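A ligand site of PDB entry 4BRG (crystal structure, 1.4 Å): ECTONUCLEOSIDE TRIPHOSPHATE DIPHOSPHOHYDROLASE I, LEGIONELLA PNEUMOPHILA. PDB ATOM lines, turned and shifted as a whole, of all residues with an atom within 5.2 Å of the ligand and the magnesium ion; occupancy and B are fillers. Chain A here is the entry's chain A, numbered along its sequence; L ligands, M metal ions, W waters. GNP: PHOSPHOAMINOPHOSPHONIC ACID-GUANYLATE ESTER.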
ATOM      1  N   ASP A  16       1.378 -14.827  -3.525  1.00  0.00           N
ATOM      2  CA  ASP A  16       2.711 -14.579  -2.939  1.00  0.00           C
ATOM      3  C   ASP A  16       3.740 -15.020  -4.002  1.00  0.00           C
ATOM      4  O   ASP A  16       3.956 -16.226  -4.187  1.00  0.00           O
ATOM      5  CB  ASP A  16       2.794 -15.445  -1.673  1.00  0.00           C
ATOM      6  CG  ASP A  16       4.183 -15.596  -1.093  1.00  0.00           C
ATOM      7  OD1 ASP A  16       5.120 -14.920  -1.544  1.00  0.00           O
ATOM      8  OD2 ASP A  16       4.370 -16.372  -0.134  1.00  0.00           O
ATOM      9  N   ALA A  17       4.387 -14.075  -4.693  1.00  0.00           N
ATOM     10  CA  ALA A  17       5.377 -14.415  -5.715  1.00  0.00           C
ATOM     11  C   ALA A  17       6.704 -14.289  -5.035  1.00  0.00           C
ATOM     12  O   ALA A  17       7.361 -13.228  -5.080  1.00  0.00           O
ATOM     13  CB  ALA A  17       5.246 -13.505  -6.941  1.00  0.00           C
ATOM     14  N   GLY A  18       7.115 -15.372  -4.360  1.00  0.00           N
ATOM     15  CA  GLY A  18       8.329 -15.419  -3.557  1.00  0.00           C
ATOM     16  C   GLY A  18       9.527 -15.808  -4.358  1.00  0.00           C
ATOM     17  O   GLY A  18       9.445 -16.180  -5.571  1.00  0.00           O
ATOM     18  N   SER A  19      10.693 -15.759  -3.722  1.00  0.00           N
ATOM     19  CA  SER A  19      11.943 -16.024  -4.449  1.00  0.00           C
ATOM     20  C   SER A  19      12.021 -17.480  -4.927  1.00  0.00           C
ATOM     21  O   SER A  19      12.636 -17.714  -5.963  1.00  0.00           O
ATOM     22  CB  SER A  19      13.138 -15.678  -3.586  1.00  0.00           C
ATOM     23  OG  SER A  19      13.280 -16.640  -2.564  1.00  0.00           O
ATOM     24  N   THR A  20      11.397 -18.446  -4.251  1.00  0.00           N
ATOM     25  CA  THR A  20      11.512 -19.843  -4.644  1.00  0.00           C
ATOM     26  C   THR A  20      10.319 -20.381  -5.401  1.00  0.00           C
ATOM     27  O   THR A  20      10.366 -21.493  -5.929  1.00  0.00           O
ATOM     28  CB  THR A  20      11.759 -20.787  -3.451  1.00  0.00           C
ATOM     29  OG1 THR A  20      10.624 -20.907  -2.631  1.00  0.00           O
ATOM     30  CG2 THR A  20      12.966 -20.348  -2.577  1.00  0.00           C
ATOM     31  N   GLY A  21       9.250 -19.588  -5.487  1.00  0.00           N
ATOM     32  CA  GLY A  21       8.011 -20.132  -6.093  1.00  0.00           C
ATOM     33  C   GLY A  21       6.877 -19.144  -5.894  1.00  0.00           C
ATOM     34  O   GLY A  21       7.014 -18.167  -5.158  1.00  0.00           O
ATOM     35  N   ARG A  23       2.644 -18.706  -4.865  1.00  0.00           N
ATOM     36  CA  ARG A  23       1.527 -19.411  -4.230  1.00  0.00           C
ATOM     37  C   ARG A  23       0.289 -18.585  -4.385  1.00  0.00           C
ATOM     38  O   ARG A  23       0.210 -17.438  -3.889  1.00  0.00           O
ATOM     39  CB  ARG A  23       1.784 -19.607  -2.739  1.00  0.00           C
ATOM     40  CG  ARG A  23       3.080 -20.338  -2.406  1.00  0.00           C
ATOM     41  CD  ARG A  23       4.188 -19.342  -2.104  1.00  0.00           C
ATOM     42  NE  ARG A  23       5.453 -19.928  -2.367  1.00  0.00           N
ATOM     43  CZ  ARG A  23       6.619 -19.386  -1.979  1.00  0.00           C
ATOM     44  NH1 ARG A  23       6.610 -18.157  -1.418  1.00  0.00           N
ATOM     45  NH2 ARG A  23       7.792 -20.016  -2.236  1.00  0.00           N
ATOM     46  N   THR A  85       7.991 -10.558  -3.813  1.00  0.00           N
ATOM     47  CA  THR A  85       8.849 -10.244  -2.687  1.00  0.00           C
ATOM     48  C   THR A  85      10.335 -10.213  -3.088  1.00  0.00           C
ATOM     49  O   THR A  85      10.699  -9.629  -4.104  1.00  0.00           O
ATOM     50  CB  THR A  85       8.479 -11.137  -1.484  1.00  0.00           C
ATOM     51  OG1 THR A  85       8.585 -12.520  -1.829  1.00  0.00           O
ATOM     52  CG2 THR A  85       6.999 -10.886  -1.020  1.00  0.00           C
ATOM     53  N   ALA A  86      11.183 -10.839  -2.282  1.00  0.00           N
ATOM     54  CA  ALA A  86      12.576 -10.599  -2.433  1.00  0.00           C
ATOM     55  C   ALA A  86      13.240 -11.072  -3.707  1.00  0.00           C
ATOM     56  O   ALA A  86      14.247 -10.469  -4.136  1.00  0.00           O
ATOM     57  CB  ALA A  86      13.320 -11.144  -1.261  1.00  0.00           C
ATOM     58  N   GLY A  87      12.694 -12.115  -4.357  1.00  0.00           N
ATOM     59  CA  GLY A  87      13.274 -12.544  -5.664  1.00  0.00           C
ATOM     60  C   GLY A  87      13.224 -11.371  -6.643  1.00  0.00           C
ATOM     61  O   GLY A  87      14.207 -11.176  -7.379  1.00  0.00           O
ATOM     62  N   GLU A 126       5.986  -6.410   3.393  1.00  0.00           N
ATOM     63  CA  GLU A 126       5.904  -7.862   3.583  1.00  0.00           C
ATOM     64  C   GLU A 126       5.897  -8.207   5.089  1.00  0.00           C
ATOM     65  O   GLU A 126       5.145  -9.081   5.517  1.00  0.00           O
ATOM     66  CB  GLU A 126       7.093  -8.496   2.864  1.00  0.00           C
ATOM     67  CG  GLU A 126       7.160 -10.029   2.823  1.00  0.00           C
ATOM     68  CD  GLU A 126       8.389 -10.456   2.045  1.00  0.00           C
ATOM     69  OE1 GLU A 126       9.253  -9.604   1.663  1.00  0.00           O
ATOM     70  OE2 GLU A 126       8.594 -11.655   1.858  1.00  0.00           O
ATOM     71  N   ASP A 153       9.797 -14.044   9.607  1.00  0.00           N
ATOM     72  CA  ASP A 153       9.562 -14.818   8.342  1.00  0.00           C
ATOM     73  C   ASP A 153      10.895 -15.109   7.768  1.00  0.00           C
ATOM     74  O   ASP A 153      11.626 -14.215   7.387  1.00  0.00           O
ATOM     75  CB  ASP A 153       8.694 -13.984   7.393  1.00  0.00           C
ATOM     76  CG  ASP A 153       8.341 -14.685   6.045  1.00  0.00           C
ATOM     77  OD1 ASP A 153       8.953 -15.731   5.742  1.00  0.00           O
ATOM     78  OD2 ASP A 153       7.444 -14.181   5.302  1.00  0.00           O
ATOM     79  N   MET A 154      11.201 -16.415   7.740  1.00  0.00           N
ATOM     80  CA  MET A 154      12.531 -16.891   7.334  1.00  0.00           C
ATOM     81  C   MET A 154      12.422 -17.313   5.854  1.00  0.00           C
ATOM     82  O   MET A 154      12.217 -18.480   5.551  1.00  0.00           O
ATOM     83  CB  MET A 154      12.951 -18.082   8.266  1.00  0.00           C
ATOM     84  CG  MET A 154      12.960 -17.711   9.766  1.00  0.00           C
ATOM     85  SD  MET A 154      14.152 -16.366  10.044  1.00  0.00           S
ATOM     86  CE  MET A 154      14.352 -16.524  11.862  1.00  0.00           C
ATOM     87  N   GLY A 155      12.540 -16.363   4.923  1.00  0.00           N
ATOM     88  CA  GLY A 155      12.347 -16.698   3.511  1.00  0.00           C
ATOM     89  C   GLY A 155      13.610 -17.139   2.832  1.00  0.00           C
ATOM     90  O   GLY A 155      14.710 -17.331   3.412  1.00  0.00           O
ATOM     91  N   GLY A 156      13.499 -17.334   1.519  1.00  0.00           N
ATOM     92  CA  GLY A 156      14.622 -17.781   0.665  1.00  0.00           C
ATOM     93  C   GLY A 156      15.609 -16.681   0.314  1.00  0.00           C
ATOM     94  O   GLY A 156      16.832 -16.958   0.203  1.00  0.00           O
ATOM     95  N   ALA A 157      15.118 -15.423   0.142  1.00  0.00           N
ATOM     96  CA  ALA A 157      16.040 -14.315  -0.231  1.00  0.00           C
ATOM     97  C   ALA A 157      16.078 -13.192   0.765  1.00  0.00           C
ATOM     98  O   ALA A 157      17.097 -12.516   0.817  1.00  0.00           O
ATOM     99  CB  ALA A 157      15.690 -13.804  -1.646  1.00  0.00           C
ATOM    100  N   SER A 158      15.000 -12.990   1.530  1.00  0.00           N
ATOM    101  CA  SER A 158      15.062 -12.025   2.620  1.00  0.00           C
ATOM    102  C   SER A 158      14.489 -12.708   3.896  1.00  0.00           C
ATOM    103  O   SER A 158      13.774 -13.708   3.806  1.00  0.00           O
ATOM    104  CB  SER A 158      14.265 -10.751   2.303  1.00  0.00           C
ATOM    105  OG  SER A 158      12.863 -10.987   2.274  1.00  0.00           O
ATOM    106  N   GLN A 160      12.287 -11.354   7.451  1.00  0.00           N
ATOM    107  CA  GLN A 160      11.614 -10.207   8.079  1.00  0.00           C
ATOM    108  C   GLN A 160      11.555 -10.417   9.574  1.00  0.00           C
ATOM    109  O   GLN A 160      11.364 -11.564  10.056  1.00  0.00           O
ATOM    110  CB  GLN A 160      10.169  -9.998   7.587  1.00  0.00           C
ATOM    111  CG  GLN A 160      10.048  -9.452   6.165  1.00  0.00           C
ATOM    112  CD  GLN A 160      10.529 -10.484   5.114  1.00  0.00           C
ATOM    113  OE1 GLN A 160      11.598 -10.292   4.503  1.00  0.00           O
ATOM    114  NE2 GLN A 160       9.783 -11.558   4.954  1.00  0.00           N
ATOM    115  N   GLN A 198      17.571 -17.750   3.313  1.00  0.00           N
ATOM    116  CA  GLN A 198      18.322 -18.979   3.373  1.00  0.00           C
ATOM    117  C   GLN A 198      19.083 -19.294   2.075  1.00  0.00           C
ATOM    118  O   GLN A 198      20.274 -19.678   2.127  1.00  0.00           O
ATOM    119  CB  GLN A 198      17.289 -20.090   3.655  1.00  0.00           C
ATOM    120  CG  GLN A 198      17.794 -21.487   3.557  1.00  0.00           C
ATOM    121  CD  GLN A 198      16.707 -22.525   3.975  1.00  0.00           C
ATOM    122  OE1 GLN A 198      15.878 -22.307   4.896  1.00  0.00           O
ATOM    123  NE2 GLN A 198      16.765 -23.633   3.351  1.00  0.00           N
ATOM    124  N   THR A 199      18.415 -19.180   0.917  1.00  0.00           N
ATOM    125  CA  THR A 199      19.094 -19.524  -0.337  1.00  0.00           C
ATOM    126  C   THR A 199      20.219 -18.554  -0.628  1.00  0.00           C
ATOM    127  O   THR A 199      21.346 -18.949  -0.929  1.00  0.00           O
ATOM    128  CB  THR A 199      18.033 -19.580  -1.479  1.00  0.00           C
ATOM    129  OG1 THR A 199      17.048 -20.581  -1.193  1.00  0.00           O
ATOM    130  CG2 THR A 199      18.735 -19.875  -2.803  1.00  0.00           C
ATOM    131  N   GLY A 265       8.011 -19.588   7.325  1.00  0.00           N
ATOM    132  CA  GLY A 265       9.100 -19.779   6.388  1.00  0.00           C
ATOM    133  C   GLY A 265       9.925 -21.001   6.676  1.00  0.00           C
ATOM    134  O   GLY A 265       9.420 -22.032   7.159  1.00  0.00           O
ATOM    135  N   GLY A 266      11.214 -20.930   6.352  1.00  0.00           N
ATOM    136  CA  GLY A 266      12.086 -22.115   6.384  1.00  0.00           C
ATOM    137  C   GLY A 266      12.290 -22.877   7.643  1.00  0.00           C
ATOM    138  O   GLY A 266      12.605 -24.083   7.613  1.00  0.00           O
ATOM    139  N   ASN A 269      10.163 -25.969   8.045  1.00  0.00           N
ATOM    140  CA  ASN A 269      10.595 -27.154   7.289  1.00  0.00           C
ATOM    141  C   ASN A 269      11.782 -27.801   7.934  1.00  0.00           C
ATOM    142  O   ASN A 269      11.831 -29.032   8.068  1.00  0.00           O
ATOM    143  CB  ASN A 269      10.924 -26.837   5.846  1.00  0.00           C
ATOM    144  CG  ASN A 269       9.769 -26.267   5.141  1.00  0.00           C
ATOM    145  OD1 ASN A 269       9.644 -25.035   4.967  1.00  0.00           O
ATOM    146  ND2 ASN A 269       8.834 -27.112   4.837  1.00  0.00           N
ATOM    147  N   LEU A 270      12.732 -26.997   8.399  1.00  0.00           N
ATOM    148  CA  LEU A 270      13.899 -27.609   9.033  1.00  0.00           C
ATOM    149  C   LEU A 270      13.466 -28.355  10.337  1.00  0.00           C
ATOM    150  O   LEU A 270      13.861 -29.480  10.562  1.00  0.00           O
ATOM    151  CB  LEU A 270      14.903 -26.530   9.405  1.00  0.00           C
ATOM    152  CG  LEU A 270      16.188 -26.987  10.121  1.00  0.00           C
ATOM    153  CD1 LEU A 270      17.027 -27.815   9.181  1.00  0.00           C
ATOM    154  CD2 LEU A 270      17.005 -25.789  10.638  1.00  0.00           C
ATOM    155  N   TYR A 313      17.047 -31.267   1.178  1.00  0.00           N
ATOM    156  CA  TYR A 313      17.678 -30.122   1.876  1.00  0.00           C
ATOM    157  C   TYR A 313      18.610 -30.585   2.952  1.00  0.00           C
ATOM    158  O   TYR A 313      19.359 -29.798   3.523  1.00  0.00           O
ATOM    159  CB  TYR A 313      16.625 -29.174   2.487  1.00  0.00           C
ATOM    160  CG  TYR A 313      16.029 -28.289   1.482  1.00  0.00           C
ATOM    161  CD1 TYR A 313      14.979 -28.750   0.685  1.00  0.00           C
ATOM    162  CD2 TYR A 313      16.536 -26.984   1.308  1.00  0.00           C
ATOM    163  CE1 TYR A 313      14.423 -27.950  -0.314  1.00  0.00           C
ATOM    164  CE2 TYR A 313      15.984 -26.138   0.347  1.00  0.00           C
ATOM    165  CZ  TYR A 313      14.916 -26.619  -0.464  1.00  0.00           C
ATOM    166  OH  TYR A 313      14.408 -25.710  -1.363  1.00  0.00           O
ATOM    167  N   TYR A 317      21.608 -29.032   6.452  1.00  0.00           N
ATOM    168  CA  TYR A 317      21.055 -28.837   7.815  1.00  0.00           C
ATOM    169  C   TYR A 317      22.077 -28.331   8.841  1.00  0.00           C
ATOM    170  O   TYR A 317      21.656 -27.726   9.864  1.00  0.00           O
ATOM    171  CB  TYR A 317      20.408 -30.107   8.308  1.00  0.00           C
ATOM    172  CG  TYR A 317      19.128 -30.481   7.657  1.00  0.00           C
ATOM    173  CD1 TYR A 317      18.507 -29.657   6.684  1.00  0.00           C
ATOM    174  CD2 TYR A 317      18.439 -31.691   8.068  1.00  0.00           C
ATOM    175  CE1 TYR A 317      17.254 -30.008   6.151  1.00  0.00           C
ATOM    176  CE2 TYR A 317      17.250 -32.066   7.510  1.00  0.00           C
ATOM    177  CZ  TYR A 317      16.650 -31.232   6.554  1.00  0.00           C
ATOM    178  OH  TYR A 317      15.428 -31.595   5.992  1.00  0.00           O
ATOM    179  N   LEU A 320      22.084 -24.689   8.126  1.00  0.00           N
ATOM    180  CA  LEU A 320      20.831 -23.994   8.447  1.00  0.00           C
ATOM    181  C   LEU A 320      20.645 -23.850   9.964  1.00  0.00           C
ATOM    182  O   LEU A 320      20.193 -22.795  10.438  1.00  0.00           O
ATOM    183  CB  LEU A 320      19.628 -24.686   7.857  1.00  0.00           C
ATOM    184  CG  LEU A 320      19.675 -24.714   6.336  1.00  0.00           C
ATOM    185  CD1 LEU A 320      18.484 -25.509   5.854  1.00  0.00           C
ATOM    186  CD2 LEU A 320      19.604 -23.300   5.784  1.00  0.00           C
ATOM    187  N   TRP A 351       2.243 -14.957   4.284  1.00  0.00           N
ATOM    188  CA  TRP A 351       1.752 -13.650   4.728  1.00  0.00           C
ATOM    189  C   TRP A 351       0.468 -13.247   4.008  1.00  0.00           C
ATOM    190  O   TRP A 351      -0.054 -12.155   4.282  1.00  0.00           O
ATOM    191  CB  TRP A 351       2.818 -12.594   4.547  1.00  0.00           C
ATOM    192  CG  TRP A 351       3.477 -12.662   3.191  1.00  0.00           C
ATOM    193  CD1 TRP A 351       4.707 -13.224   2.932  1.00  0.00           C
ATOM    194  CD2 TRP A 351       2.993 -12.166   1.933  1.00  0.00           C
ATOM    195  NE1 TRP A 351       5.027 -13.143   1.599  1.00  0.00           N
ATOM    196  CE2 TRP A 351       3.993 -12.495   0.939  1.00  0.00           C
ATOM    197  CE3 TRP A 351       1.830 -11.467   1.533  1.00  0.00           C
ATOM    198  CZ2 TRP A 351       3.823 -12.211  -0.416  1.00  0.00           C
ATOM    199  CZ3 TRP A 351       1.673 -11.147   0.177  1.00  0.00           C
ATOM    200  CH2 TRP A 351       2.651 -11.507  -0.796  1.00  0.00           C
HETATM  201  PG  GNP L   1      11.164 -14.911  -0.085  1.00  0.00           P
HETATM  202  O1G GNP L   1      10.747 -14.186  -1.389  1.00  0.00           O
HETATM  203  O2G GNP L   1      10.103 -14.794   0.971  1.00  0.00           O
HETATM  204  O3G GNP L   1      12.563 -14.453   0.398  1.00  0.00           O
HETATM  205  N3B GNP L   1      11.318 -16.536  -0.477  1.00  0.00           N
HETATM  206  PB  GNP L   1      10.144 -17.711  -0.412  1.00  0.00           P
HETATM  207  O1B GNP L   1       8.869 -17.157   0.094  1.00  0.00           O
HETATM  208  O2B GNP L   1      10.103 -18.406  -1.719  1.00  0.00           O
HETATM  209  O3A GNP L   1      10.751 -18.686   0.707  1.00  0.00           O
HETATM  210  PA  GNP L   1       9.937 -19.870   1.461  1.00  0.00           P
HETATM  211  O1A GNP L   1       8.956 -20.554   0.556  1.00  0.00           O
HETATM  212  O2A GNP L   1       9.483 -19.352   2.777  1.00  0.00           O
HETATM  213  O5' GNP L   1      11.126 -20.876   1.762  1.00  0.00           O
HETATM  214  C5' GNP L   1      11.984 -20.604   2.796  1.00  0.00           C
HETATM  215  C4' GNP L   1      13.274 -21.385   2.544  1.00  0.00           C
HETATM  216  O4' GNP L   1      12.891 -22.758   2.780  1.00  0.00           O
HETATM  217  C3' GNP L   1      13.836 -21.331   1.108  1.00  0.00           C
HETATM  218  O3' GNP L   1      15.271 -21.108   1.236  1.00  0.00           O
HETATM  219  C2' GNP L   1      13.517 -22.713   0.533  1.00  0.00           C
HETATM  220  O2' GNP L   1      14.533 -23.006  -0.431  1.00  0.00           O
HETATM  221  C1' GNP L   1      13.566 -23.534   1.764  1.00  0.00           C
HETATM  222  N9  GNP L   1      12.894 -24.807   1.700  1.00  0.00           N
HETATM  223  C8  GNP L   1      11.900 -25.249   0.884  1.00  0.00           C
HETATM  224  N7  GNP L   1      11.541 -26.527   1.161  1.00  0.00           N
HETATM  225  C5  GNP L   1      12.333 -26.929   2.199  1.00  0.00           C
HETATM  226  C6  GNP L   1      12.565 -28.124   3.001  1.00  0.00           C
HETATM  227  O6  GNP L   1      11.892 -29.126   2.805  1.00  0.00           O
HETATM  228  N1  GNP L   1      13.494 -28.058   3.975  1.00  0.00           N
HETATM  229  C2  GNP L   1      14.296 -26.999   4.244  1.00  0.00           C
HETATM  230  N2  GNP L   1      15.178 -27.064   5.284  1.00  0.00           N
HETATM  231  N3  GNP L   1      14.136 -25.848   3.550  1.00  0.00           N
HETATM  232  C4  GNP L   1      13.216 -25.782   2.542  1.00  0.00           C
HETATM  233 MG    MG M   1       8.328 -15.617   1.358  1.00  0.00          MG
HETATM  234  O   HOH W   1      15.114 -23.014  -3.239  1.00  0.00           O
HETATM  235  O   HOH W   2       6.493 -19.316   1.796  1.00  0.00           O
HETATM  236  O   HOH W   3      10.067 -23.179  -1.101  1.00  0.00           O
HETATM  237  O   HOH W   4      12.823 -31.817   3.483  1.00  0.00           O
HETATM  238  O   HOH W   5      10.897 -13.683   3.404  1.00  0.00           O
HETATM  239  O   HOH W   6       6.402 -16.529   1.589  1.00  0.00           O
HETATM  240  O   HOH W   7       8.862 -16.695   3.050  1.00  0.00           O
HETATM  241  O   HOH W   8      10.880 -11.816   0.508  1.00  0.00           O
HETATM  242  O   HOH W   9      15.144 -24.502   6.468  1.00  0.00           O
HETATM  243  O   HOH W  10       7.370 -14.487  -0.139  1.00  0.00           O
HETATM  244  O   HOH W  11       7.832 -14.072   2.672  1.00  0.00           O
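An oxygen (O2B) of the ligand is in hydrogen-bond range of the backbone NH (N) of Thr 20 (2.8 Å). The backbone NH of Gly 156 sits at hydrogen-bond distance from an oxygen (O3A) of the ligand (3.2 Å). N3 of the ligand sits at hydrogen-bond distance from NE2 of Gln 198 (3.4 Å). The side-chain hydroxyl (OG) of Ser 19 lies within hydrogen-bond range of a nitrogen (N3B) of the ligand. N of Ala 86 sits at hydrogen-bond distance from O1G of the ligand. The backbone NH (N) of Ala 157 lies within hydrogen-bond range of an oxygen (O3G) of the ligand, at 2.7 Å. An oxygen (O3') of the ligand is in hydrogen-bond range of the side-chain hydroxyl (OG1) of Thr 199 (3.1 Å). N of Ser 19 is in hydrogen-bond range of O1G of the ligand (2.8 Å). An oxygen (O3G) of the ligand sits at hydrogen-bond distance from the backbone NH of Ser 158, at 3.1 Å. The guanidinium group (NH2) of Arg 23 is in salt-bridge range of an oxygen (O2B) of the ligand. The side-chain hydroxyl (OH) of Tyr 313 is in hydrogen-bond range of an oxygen (O2') of the ligand (2.9 Å). The side-chain hydroxyl of Thr 85 lies within hydrogen-bond range of an oxygen (O1G) of the ligand. An oxygen (O2B) of the ligand is in hydrogen-bond range of the side-chain hydroxyl (OG1) of Thr 20.
The side-chain carboxylate (OE2) of Glu 126 lies within hydrogen-bond range of the side-chain amide nitrogen (NE2) of Gln 160, at 3.3 Å. The side-chain hydroxyl (OG) of Ser 158 sits at hydrogen-bond distance from the side-chain amide oxygen (OE1) of Gln 160, 2.7 Å away. The backbone NH (N) of Gln 198 is in hydrogen-bond range of the backbone carbonyl oxygen (O) of Gly 155 (2.9 Å). The backbone NH (N) of Thr 85 is in hydrogen-bond range of the backbone carbonyl oxygen (O) of Ala 17 (3.0 Å). OD1 of Asp 16 lies close to N of Gly 18 (3.5 Å). OG1 of Thr 20 is in hydrogen-bond range of NH2 of Arg 23, 3.0 Å away. The guanidinium group (NH1) of Arg 23 lies within salt-bridge range of the side-chain carboxylate (OD2) of Asp 16, at 3.1 Å. The backbone carbonyl oxygen of Met 154 is in hydrogen-bond range of the backbone NH of Gly 266, at 2.8 Å.
Residues that only touch the ligand: Asn 269 (3.4 Å), Gly 18 (3.5 Å), Met 154 (3.5 Å), Glu 126 (3.6 Å), Gly 266 (3.7 Å), Gly 265 (3.7 Å), Leu 320 (3.7 Å), Tyr 317 (3.7 Å), Gly 155 (3.8 Å) and Leu 270 (3.96 Å). The nearest printed residue that does not touch the ligand is Gly 21 (4.04 Å).
No residue comes within 4 Å of the magnesium ion. The nearest printed residue that does not touch the magnesium ion is Glu 126 (4.002 Å).
The magnesium ion is bound by O2G of the ligand, O1B of the ligand, water W7, water W11, water W10 and water W6. The magnesium ion has six donor atoms within binding distance.
Water W10 lies within hydrogen-bond range of the side-chain carboxylate (OD1) of Asp 16 (2.7 Å), the side-chain hydroxyl (OG1) of Thr 85 (2.9 Å) and the indole nitrogen (NE1) of Trp 351 (3.2 Å). Water W5 lies within hydrogen-bond range of the side-chain amide nitrogen of Gln 160, the backbone carbonyl oxygen of Ser 158, the side-chain carboxylate of Glu 126 and the backbone NH of Gly 155. Water W9 lies within hydrogen-bond range of the side-chain amide oxygen (OE1) of Gln 198 (2.8 Å), the backbone carbonyl oxygen (O) of Gly 266 (2.8 Å) and a nitrogen (N2) of the ligand (2.8 Å). Water W1 bridges an oxygen (O2') of the ligand (2.9 Å) and the side-chain hydroxyl (OH) of Tyr 313 (3.4 Å). Water W8 lies within hydrogen-bond range of OE2 of Glu 126 (2.7 Å), OG of Ser 158 (2.8 Å), N of Ala 86 (3.0 Å), O1G of the ligand (3.0 Å) and OG1 of Thr 85 (3.4 Å). Water W3 bridges the side-chain hydroxyl of Thr 20 (2.8 Å) and an oxygen (O1A) of the ligand (3.3 Å).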
